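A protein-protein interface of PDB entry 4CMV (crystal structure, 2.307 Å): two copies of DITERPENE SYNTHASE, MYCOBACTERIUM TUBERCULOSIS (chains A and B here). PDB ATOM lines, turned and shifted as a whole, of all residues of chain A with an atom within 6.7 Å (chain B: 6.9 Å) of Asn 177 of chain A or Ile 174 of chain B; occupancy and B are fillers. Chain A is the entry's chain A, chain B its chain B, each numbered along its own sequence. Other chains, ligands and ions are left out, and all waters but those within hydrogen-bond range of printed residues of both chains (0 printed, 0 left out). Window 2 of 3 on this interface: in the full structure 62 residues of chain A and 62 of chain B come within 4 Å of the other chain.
Ala 170 of chain A touches Ser 173 of chain B, and with the chains exchanged Ser 173 of chain A touches Ala 170 of chain B.
Ser 173 of chain A touches Ile 174 of chain B, and with the chains exchanged Ile 174 of chain A touches Ser 173 of chain B.
Ile 174 of chain A touches Asn 177 of chain B, and with the chains exchanged Asn 177 of chain A touches Ile 174 of chain B.
10 positions are printed for both chains.
Of the 8 pairs that touch across the chains among the printed residues, 6 have their exchanged pair printed and touching as well.
Printed residues of chain B within 4 Å of Asn 177 of chain A: Ile 174.
Of chain A, only Ser 173, Asn 177 and Pro 183 come within 4 Å of Ile 174 of chain B.
Of the printed residues of chain B, Ser 173 of chain A touches Ala 170 (3.2 Å) and Ile 174 (3.5 Å).
Of the printed residues of chain A, Ser 173 of chain B touches Ala 170 (3.3 Å) and Ile 174 (3.6 Å).
Of the printed residues of chain A, Gln 171 of chain B touches Pro 183.
Of the printed residues of chain B, Pro 183 of chain A touches Gln 171 and Ile 174.
The nearest residue of chain B that does not touch Asn 177 of chain A is Glu 178 of chain B (4.4 Å).
Among the printed residues, pairs that only touch across the chains: Ala 170 of chain A with Ser 173 of chain B (3.3 Å), Ser 173 of chain A with Ala 170 of chain B (3.2 Å), Ser 173 of chain A with Ile 174 of chain B (3.5 Å), Ile 174 of chain A with Ser 173 of chain B (3.6 Å), Ile 174 of chain A with Asn 177 of chain B (3.6 Å), Asn 177 of chain A with Ile 174 of chain B (3.6 Å), Pro 183 of chain A with Gln 171 of chain B (3.96 Å) and Pro 183 of chain A with Ile 174 of chain B (3.8 Å).
The backbone carbonyl oxygen (O) of Val 169 of chain B is in hydrogen-bond range of the side-chain hydroxyl (OG) of Ser 173 of chain B (2.7 Å).
Of the 13 printed residues of chain B, 5 touch a printed residue of chain A.
Of the 14 printed residues of chain A, 5 touch a printed residue of chain B.
Hydrophobic or aromatic side chains of chain A within 4 Å of the printed part of chain B: Ala 170, Ile 174 and Pro 183.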
ATOM      1  N   ALA A 170      19.177  -1.606  22.145  1.00  0.00           N
ATOM      2  CA  ALA A 170      20.188  -1.033  23.040  1.00  0.00           C
ATOM      3  C   ALA A 170      20.117   0.486  23.087  1.00  0.00           C
ATOM      4  O   ALA A 170      20.044   1.099  24.169  1.00  0.00           O
ATOM      5  CB  ALA A 170      21.596  -1.476  22.618  1.00  0.00           C
ATOM      6  N   PHE A 172      17.688   2.488  21.923  1.00  0.00           N
ATOM      7  CA  PHE A 172      16.367   2.864  22.423  1.00  0.00           C
ATOM      8  C   PHE A 172      16.327   2.816  23.955  1.00  0.00           C
ATOM      9  O   PHE A 172      15.801   3.719  24.582  1.00  0.00           O
ATOM     10  CB  PHE A 172      15.281   1.949  21.830  1.00  0.00           C
ATOM     11  CG  PHE A 172      13.932   2.125  22.460  1.00  0.00           C
ATOM     12  CD1 PHE A 172      13.577   1.394  23.590  1.00  0.00           C
ATOM     13  CD2 PHE A 172      13.016   3.023  21.930  1.00  0.00           C
ATOM     14  CE1 PHE A 172      12.323   1.572  24.198  1.00  0.00           C
ATOM     15  CE2 PHE A 172      11.776   3.201  22.527  1.00  0.00           C
ATOM     16  CZ  PHE A 172      11.429   2.472  23.662  1.00  0.00           C
ATOM     17  N   SER A 173      16.881   1.756  24.543  1.00  0.00           N
ATOM     18  CA  SER A 173      16.818   1.563  25.975  1.00  0.00           C
ATOM     19  C   SER A 173      17.658   2.595  26.685  1.00  0.00           C
ATOM     20  O   SER A 173      17.260   3.083  27.736  1.00  0.00           O
ATOM     21  CB  SER A 173      17.288   0.162  26.378  1.00  0.00           C
ATOM     22  OG  SER A 173      16.461  -0.848  25.821  1.00  0.00           O
ATOM     23  N   ILE A 174      18.825   2.913  26.123  1.00  0.00           N
ATOM     24  CA  ILE A 174      19.680   3.943  26.704  1.00  0.00           C
ATOM     25  C   ILE A 174      18.983   5.306  26.703  1.00  0.00           C
ATOM     26  O   ILE A 174      18.904   5.993  27.760  1.00  0.00           O
ATOM     27  CB  ILE A 174      21.027   4.019  25.959  1.00  0.00           C
ATOM     28  CG1 ILE A 174      21.875   2.792  26.309  1.00  0.00           C
ATOM     29  CG2 ILE A 174      21.794   5.280  26.346  1.00  0.00           C
ATOM     30  CD1 ILE A 174      22.960   2.460  25.307  1.00  0.00           C
ATOM     31  N   SER A 175      18.434   5.684  25.545  1.00  0.00           N
ATOM     32  CA  SER A 175      17.728   6.965  25.466  1.00  0.00           C
ATOM     33  C   SER A 175      16.580   6.974  26.455  1.00  0.00           C
ATOM     34  O   SER A 175      16.381   7.940  27.194  1.00  0.00           O
ATOM     35  CB  SER A 175      17.168   7.218  24.063  1.00  0.00           C
ATOM     36  OG  SER A 175      18.188   7.324  23.097  1.00  0.00           O
ATOM     37  N   TRP A 176      15.858   5.863  26.494  1.00  0.00           N
ATOM     38  CA  TRP A 176      14.698   5.756  27.354  1.00  0.00           C
ATOM     39  C   TRP A 176      15.092   5.951  28.805  1.00  0.00           C
ATOM     40  O   TRP A 176      14.408   6.662  29.552  1.00  0.00           O
ATOM     41  CB  TRP A 176      14.008   4.410  27.182  1.00  0.00           C
ATOM     42  CG  TRP A 176      12.724   4.343  27.928  1.00  0.00           C
ATOM     43  CD1 TRP A 176      12.554   4.081  29.271  1.00  0.00           C
ATOM     44  CD2 TRP A 176      11.404   4.532  27.382  1.00  0.00           C
ATOM     45  NE1 TRP A 176      11.211   4.098  29.587  1.00  0.00           N
ATOM     46  CE2 TRP A 176      10.484   4.372  28.446  1.00  0.00           C
ATOM     47  CE3 TRP A 176      10.914   4.817  26.099  1.00  0.00           C
ATOM     48  CZ2 TRP A 176       9.097   4.498  28.258  1.00  0.00           C
ATOM     49  CZ3 TRP A 176       9.544   4.934  25.916  1.00  0.00           C
ATOM     50  CH2 TRP A 176       8.651   4.779  26.986  1.00  0.00           C
ATOM     51  N   ASN A 177      16.186   5.323  29.212  1.00  0.00           N
ATOM     52  CA  ASN A 177      16.632   5.470  30.585  1.00  0.00           C
ATOM     53  C   ASN A 177      16.984   6.920  30.895  1.00  0.00           C
ATOM     54  O   ASN A 177      16.595   7.457  31.940  1.00  0.00           O
ATOM     55  CB  ASN A 177      17.830   4.574  30.860  1.00  0.00           C
ATOM     56  CG  ASN A 177      18.241   4.588  32.316  1.00  0.00           C
ATOM     57  OD1 ASN A 177      17.603   3.953  33.158  1.00  0.00           O
ATOM     58  ND2 ASN A 177      19.319   5.304  32.622  1.00  0.00           N
ATOM     59  N   GLU A 178      17.707   7.565  29.985  1.00  0.00           N
ATOM     60  CA  GLU A 178      18.054   8.958  30.230  1.00  0.00           C
ATOM     61  C   GLU A 178      16.815   9.889  30.309  1.00  0.00           C
ATOM     62  O   GLU A 178      16.747  10.787  31.147  1.00  0.00           O
ATOM     63  CB  GLU A 178      19.058   9.460  29.191  1.00  0.00           C
ATOM     64  CG  GLU A 178      19.478  10.918  29.396  1.00  0.00           C
ATOM     65  CD  GLU A 178      20.050  11.270  30.801  1.00  0.00           C
ATOM     66  OE1 GLU A 178      19.505  10.858  31.855  1.00  0.00           O
ATOM     67  OE2 GLU A 178      21.058  12.009  30.848  1.00  0.00           O
ATOM     68  N   THR A 179      15.819   9.644  29.471  1.00  0.00           N
ATOM     69  CA  THR A 179      14.621  10.471  29.433  1.00  0.00           C
ATOM     70  C   THR A 179      13.685  10.204  30.639  1.00  0.00           C
ATOM     71  O   THR A 179      13.288  11.140  31.340  1.00  0.00           O
ATOM     72  CB  THR A 179      13.861  10.228  28.103  1.00  0.00           C
ATOM     73  OG1 THR A 179      14.706  10.582  26.994  1.00  0.00           O
ATOM     74  CG2 THR A 179      12.570  11.030  28.036  1.00  0.00           C
ATOM     75  N   HIS A 180      13.274   8.958  30.859  1.00  0.00           N
ATOM     76  CA  HIS A 180      12.237   8.661  31.851  1.00  0.00           C
ATOM     77  C   HIS A 180      12.800   8.236  33.181  1.00  0.00           C
ATOM     78  O   HIS A 180      12.064   7.909  34.111  1.00  0.00           O
ATOM     79  CB  HIS A 180      11.343   7.559  31.314  1.00  0.00           C
ATOM     80  CG  HIS A 180      10.872   7.834  29.952  1.00  0.00           C
ATOM     81  ND1 HIS A 180      11.693   7.668  28.861  1.00  0.00           N
ATOM     82  CD2 HIS A 180       9.685   8.302  29.471  1.00  0.00           C
ATOM     83  CE1 HIS A 180      11.035   8.002  27.773  1.00  0.00           C
ATOM     84  NE2 HIS A 180       9.811   8.390  28.119  1.00  0.00           N
ATOM     85  N   GLY A 181      14.115   8.277  33.287  1.00  0.00           N
ATOM     86  CA  GLY A 181      14.714   7.933  34.554  1.00  0.00           C
ATOM     87  C   GLY A 181      14.803   6.444  34.851  1.00  0.00           C
ATOM     88  O   GLY A 181      15.332   6.073  35.888  1.00  0.00           O
ATOM     89  N   LYS A 182      14.285   5.575  33.994  1.00  0.00           N
ATOM     90  CA  LYS A 182      14.297   4.152  34.342  1.00  0.00           C
ATOM     91  C   LYS A 182      14.312   3.295  33.068  1.00  0.00           C
ATOM     92  O   LYS A 182      14.096   3.839  31.985  1.00  0.00           O
ATOM     93  CB  LYS A 182      13.072   3.829  35.200  1.00  0.00           C
ATOM     94  CG  LYS A 182      11.760   4.241  34.533  1.00  0.00           C
ATOM     95  CD  LYS A 182      10.678   4.550  35.561  1.00  0.00           C
ATOM     96  CE  LYS A 182       9.473   5.208  34.904  1.00  0.00           C
ATOM     97  NZ  LYS A 182       8.332   5.316  35.858  1.00  0.00           N
ATOM     98  N   PRO A 183      14.569   1.962  33.186  1.00  0.00           N
ATOM     99  CA  PRO A 183      14.548   1.093  31.988  1.00  0.00           C
ATOM    100  C   PRO A 183      13.154   0.868  31.415  1.00  0.00           C
ATOM    101  O   PRO A 183      12.172   0.826  32.157  1.00  0.00           O
ATOM    102  CB  PRO A 183      15.140  -0.239  32.487  1.00  0.00           C
ATOM    103  CG  PRO A 183      14.966  -0.223  33.994  1.00  0.00           C
ATOM    104  CD  PRO A 183      15.071   1.245  34.383  1.00  0.00           C
ATOM    105  N   PRO A 184      13.057   0.749  30.085  1.00  0.00           N
ATOM    106  CA  PRO A 184      11.778   0.447  29.443  1.00  0.00           C
ATOM    107  C   PRO A 184      11.354  -0.992  29.701  1.00  0.00           C
ATOM    108  O   PRO A 184      12.202  -1.881  29.849  1.00  0.00           O
ATOM    109  CB  PRO A 184      12.078   0.646  27.956  1.00  0.00           C
ATOM    110  CG  PRO A 184      13.517   0.251  27.833  1.00  0.00           C
ATOM    111  CD  PRO A 184      14.168   0.759  29.113  1.00  0.00           C
ATOM    112  N   GLU B 167      14.117  -7.180  27.968  1.00  0.00           N
ATOM    113  CA  GLU B 167      14.424  -6.398  29.184  1.00  0.00           C
ATOM    114  C   GLU B 167      15.848  -6.639  29.713  1.00  0.00           C
ATOM    115  O   GLU B 167      16.510  -5.711  30.196  1.00  0.00           O
ATOM    116  CB  GLU B 167      13.374  -6.685  30.272  1.00  0.00           C
ATOM    117  CG  GLU B 167      11.990  -6.118  29.895  1.00  0.00           C
ATOM    118  CD  GLU B 167      10.929  -6.289  30.985  1.00  0.00           C
ATOM    119  OE1 GLU B 167      11.254  -6.821  32.071  1.00  0.00           O
ATOM    120  OE2 GLU B 167       9.769  -5.882  30.747  1.00  0.00           O
ATOM    121  N   VAL B 169      18.442  -7.253  27.822  1.00  0.00           N
ATOM    122  CA  VAL B 169      19.272  -6.470  26.899  1.00  0.00           C
ATOM    123  C   VAL B 169      19.144  -4.981  27.182  1.00  0.00           C
ATOM    124  O   VAL B 169      20.120  -4.239  27.138  1.00  0.00           O
ATOM    125  CB  VAL B 169      18.887  -6.764  25.433  1.00  0.00           C
ATOM    126  CG1 VAL B 169      19.444  -5.717  24.489  1.00  0.00           C
ATOM    127  CG2 VAL B 169      19.352  -8.119  25.046  1.00  0.00           C
ATOM    128  N   ALA B 170      17.936  -4.549  27.511  1.00  0.00           N
ATOM    129  CA  ALA B 170      17.719  -3.165  27.865  1.00  0.00           C
ATOM    130  C   ALA B 170      18.607  -2.779  29.034  1.00  0.00           C
ATOM    131  O   ALA B 170      19.418  -1.834  28.944  1.00  0.00           O
ATOM    132  CB  ALA B 170      16.253  -2.931  28.205  1.00  0.00           C
ATOM    133  N   GLN B 171      18.479  -3.531  30.123  1.00  0.00           N
ATOM    134  CA  GLN B 171      19.235  -3.196  31.325  1.00  0.00           C
ATOM    135  C   GLN B 171      20.728  -3.283  31.071  1.00  0.00           C
ATOM    136  O   GLN B 171      21.470  -2.354  31.407  1.00  0.00           O
ATOM    137  CB  GLN B 171      18.848  -4.107  32.491  1.00  0.00           C
ATOM    138  CG  GLN B 171      19.675  -3.860  33.761  1.00  0.00           C
ATOM    139  CD  GLN B 171      19.615  -2.413  34.244  1.00  0.00           C
ATOM    140  OE1 GLN B 171      20.617  -1.677  34.205  1.00  0.00           O
ATOM    141  NE2 GLN B 171      18.434  -1.999  34.711  1.00  0.00           N
ATOM    142  N   PHE B 172      21.150  -4.378  30.438  1.00  0.00           N
ATOM    143  CA  PHE B 172      22.552  -4.562  30.069  1.00  0.00           C
ATOM    144  C   PHE B 172      23.086  -3.349  29.320  1.00  0.00           C
ATOM    145  O   PHE B 172      24.146  -2.857  29.634  1.00  0.00           O
ATOM    146  CB  PHE B 172      22.726  -5.814  29.204  1.00  0.00           C
ATOM    147  CG  PHE B 172      24.118  -5.964  28.612  1.00  0.00           C
ATOM    148  CD1 PHE B 172      25.124  -6.640  29.313  1.00  0.00           C
ATOM    149  CD2 PHE B 172      24.417  -5.448  27.352  1.00  0.00           C
ATOM    150  CE1 PHE B 172      26.405  -6.778  28.768  1.00  0.00           C
ATOM    151  CE2 PHE B 172      25.695  -5.577  26.799  1.00  0.00           C
ATOM    152  CZ  PHE B 172      26.686  -6.246  27.503  1.00  0.00           C
ATOM    153  N   SER B 173      22.332  -2.855  28.351  1.00  0.00           N
ATOM    154  CA  SER B 173      22.796  -1.769  27.502  1.00  0.00           C
ATOM    155  C   SER B 173      22.863  -0.464  28.279  1.00  0.00           C
ATOM    156  O   SER B 173      23.796   0.330  28.096  1.00  0.00           O
ATOM    157  CB  SER B 173      21.878  -1.636  26.286  1.00  0.00           C
ATOM    158  OG  SER B 173      21.861  -2.859  25.554  1.00  0.00           O
ATOM    159  N   ILE B 174      21.885  -0.235  29.153  1.00  0.00           N
ATOM    160  CA  ILE B 174      21.921   0.964  29.999  1.00  0.00           C
ATOM    161  C   ILE B 174      23.170   0.971  30.891  1.00  0.00           C
ATOM    162  O   ILE B 174      23.917   1.979  30.982  1.00  0.00           O
ATOM    163  CB  ILE B 174      20.631   1.049  30.841  1.00  0.00           C
ATOM    164  CG1 ILE B 174      19.452   1.385  29.924  1.00  0.00           C
ATOM    165  CG2 ILE B 174      20.744   2.092  31.951  1.00  0.00           C
ATOM    166  CD1 ILE B 174      18.099   0.929  30.456  1.00  0.00           C
ATOM    167  N   SER B 175      23.408  -0.164  31.540  1.00  0.00           N
ATOM    168  CA  SER B 175      24.585  -0.320  32.400  1.00  0.00           C
ATOM    169  C   SER B 175      25.891  -0.194  31.611  1.00  0.00           C
ATOM    170  O   SER B 175      26.851   0.437  32.066  1.00  0.00           O
ATOM    171  CB  SER B 175      24.525  -1.666  33.125  1.00  0.00           C
ATOM    172  OG  SER B 175      25.824  -2.113  33.470  1.00  0.00           O
ATOM    173  N   TRP B 176      25.912  -0.786  30.419  1.00  0.00           N
ATOM    174  CA  TRP B 176      27.096  -0.779  29.568  1.00  0.00           C
ATOM    175  C   TRP B 176      27.442   0.637  29.195  1.00  0.00           C
ATOM    176  O   TRP B 176      28.576   1.078  29.382  1.00  0.00           O
ATOM    177  CB  TRP B 176      26.873  -1.612  28.302  1.00  0.00           C
ATOM    178  CG  TRP B 176      28.130  -1.777  27.450  1.00  0.00           C
ATOM    179  CD1 TRP B 176      28.629  -0.886  26.540  1.00  0.00           C
ATOM    180  CD2 TRP B 176      29.026  -2.908  27.432  1.00  0.00           C
ATOM    181  NE1 TRP B 176      29.775  -1.386  25.963  1.00  0.00           N
ATOM    182  CE2 TRP B 176      30.044  -2.624  26.496  1.00  0.00           C
ATOM    183  CE3 TRP B 176      29.067  -4.132  28.125  1.00  0.00           C
ATOM    184  CZ2 TRP B 176      31.092  -3.524  26.227  1.00  0.00           C
ATOM    185  CZ3 TRP B 176      30.106  -5.025  27.853  1.00  0.00           C
ATOM    186  CH2 TRP B 176      31.105  -4.713  26.913  1.00  0.00           C
ATOM    187  N   ASN B 177      26.434   1.373  28.736  1.00  0.00           N
ATOM    188  CA  ASN B 177      26.641   2.758  28.342  1.00  0.00           C
ATOM    189  C   ASN B 177      27.150   3.567  29.526  1.00  0.00           C
ATOM    190  O   ASN B 177      28.065   4.384  29.367  1.00  0.00           O
ATOM    191  CB  ASN B 177      25.357   3.377  27.797  1.00  0.00           C
ATOM    192  CG  ASN B 177      25.580   4.778  27.223  1.00  0.00           C
ATOM    193  OD1 ASN B 177      26.070   4.928  26.100  1.00  0.00           O
ATOM    194  ND2 ASN B 177      25.231   5.811  27.999  1.00  0.00           N
ATOM    195  N   GLU B 178      26.576   3.333  30.711  1.00  0.00           N
ATOM    196  CA  GLU B 178      27.079   4.023  31.900  1.00  0.00           C
ATOM    197  C   GLU B 178      28.555   3.743  32.164  1.00  0.00           C
ATOM    198  O   GLU B 178      29.312   4.671  32.414  1.00  0.00           O
ATOM    199  CB  GLU B 178      26.298   3.610  33.152  1.00  0.00           C
ATOM    200  CG  GLU B 178      24.887   4.149  33.274  1.00  0.00           C
ATOM    201  CD  GLU B 178      24.081   3.400  34.340  1.00  0.00           C
ATOM    202  OE1 GLU B 178      24.549   2.338  34.820  1.00  0.00           O
ATOM    203  OE2 GLU B 178      22.973   3.871  34.694  1.00  0.00           O
ATOM    204  N   THR B 179      28.955   2.469  32.139  1.00  0.00           N
ATOM    205  CA  THR B 179      30.352   2.119  32.461  1.00  0.00           C
ATOM    206  C   THR B 179      31.279   2.007  31.260  1.00  0.00           C
ATOM    207  O   THR B 179      32.251   2.746  31.160  1.00  0.00           O
ATOM    208  CB  THR B 179      30.464   0.788  33.230  1.00  0.00           C
ATOM    209  OG1 THR B 179      30.103  -0.278  32.367  1.00  0.00           O
ATOM    210  CG2 THR B 179      29.551   0.761  34.413  1.00  0.00           C
ATOM    211  N   PRO B 184      26.706  -0.783  23.641  1.00  0.00           N
ATOM    212  CA  PRO B 184      27.359  -2.055  23.334  1.00  0.00           C
ATOM    213  C   PRO B 184      27.005  -2.471  21.922  1.00  0.00           C
ATOM    214  O   PRO B 184      25.878  -2.202  21.491  1.00  0.00           O
ATOM    215  CB  PRO B 184      26.751  -3.012  24.350  1.00  0.00           C
ATOM    216  CG  PRO B 184      25.361  -2.472  24.542  1.00  0.00           C
ATOM    217  CD  PRO B 184      25.502  -0.965  24.474  1.00  0.00           C
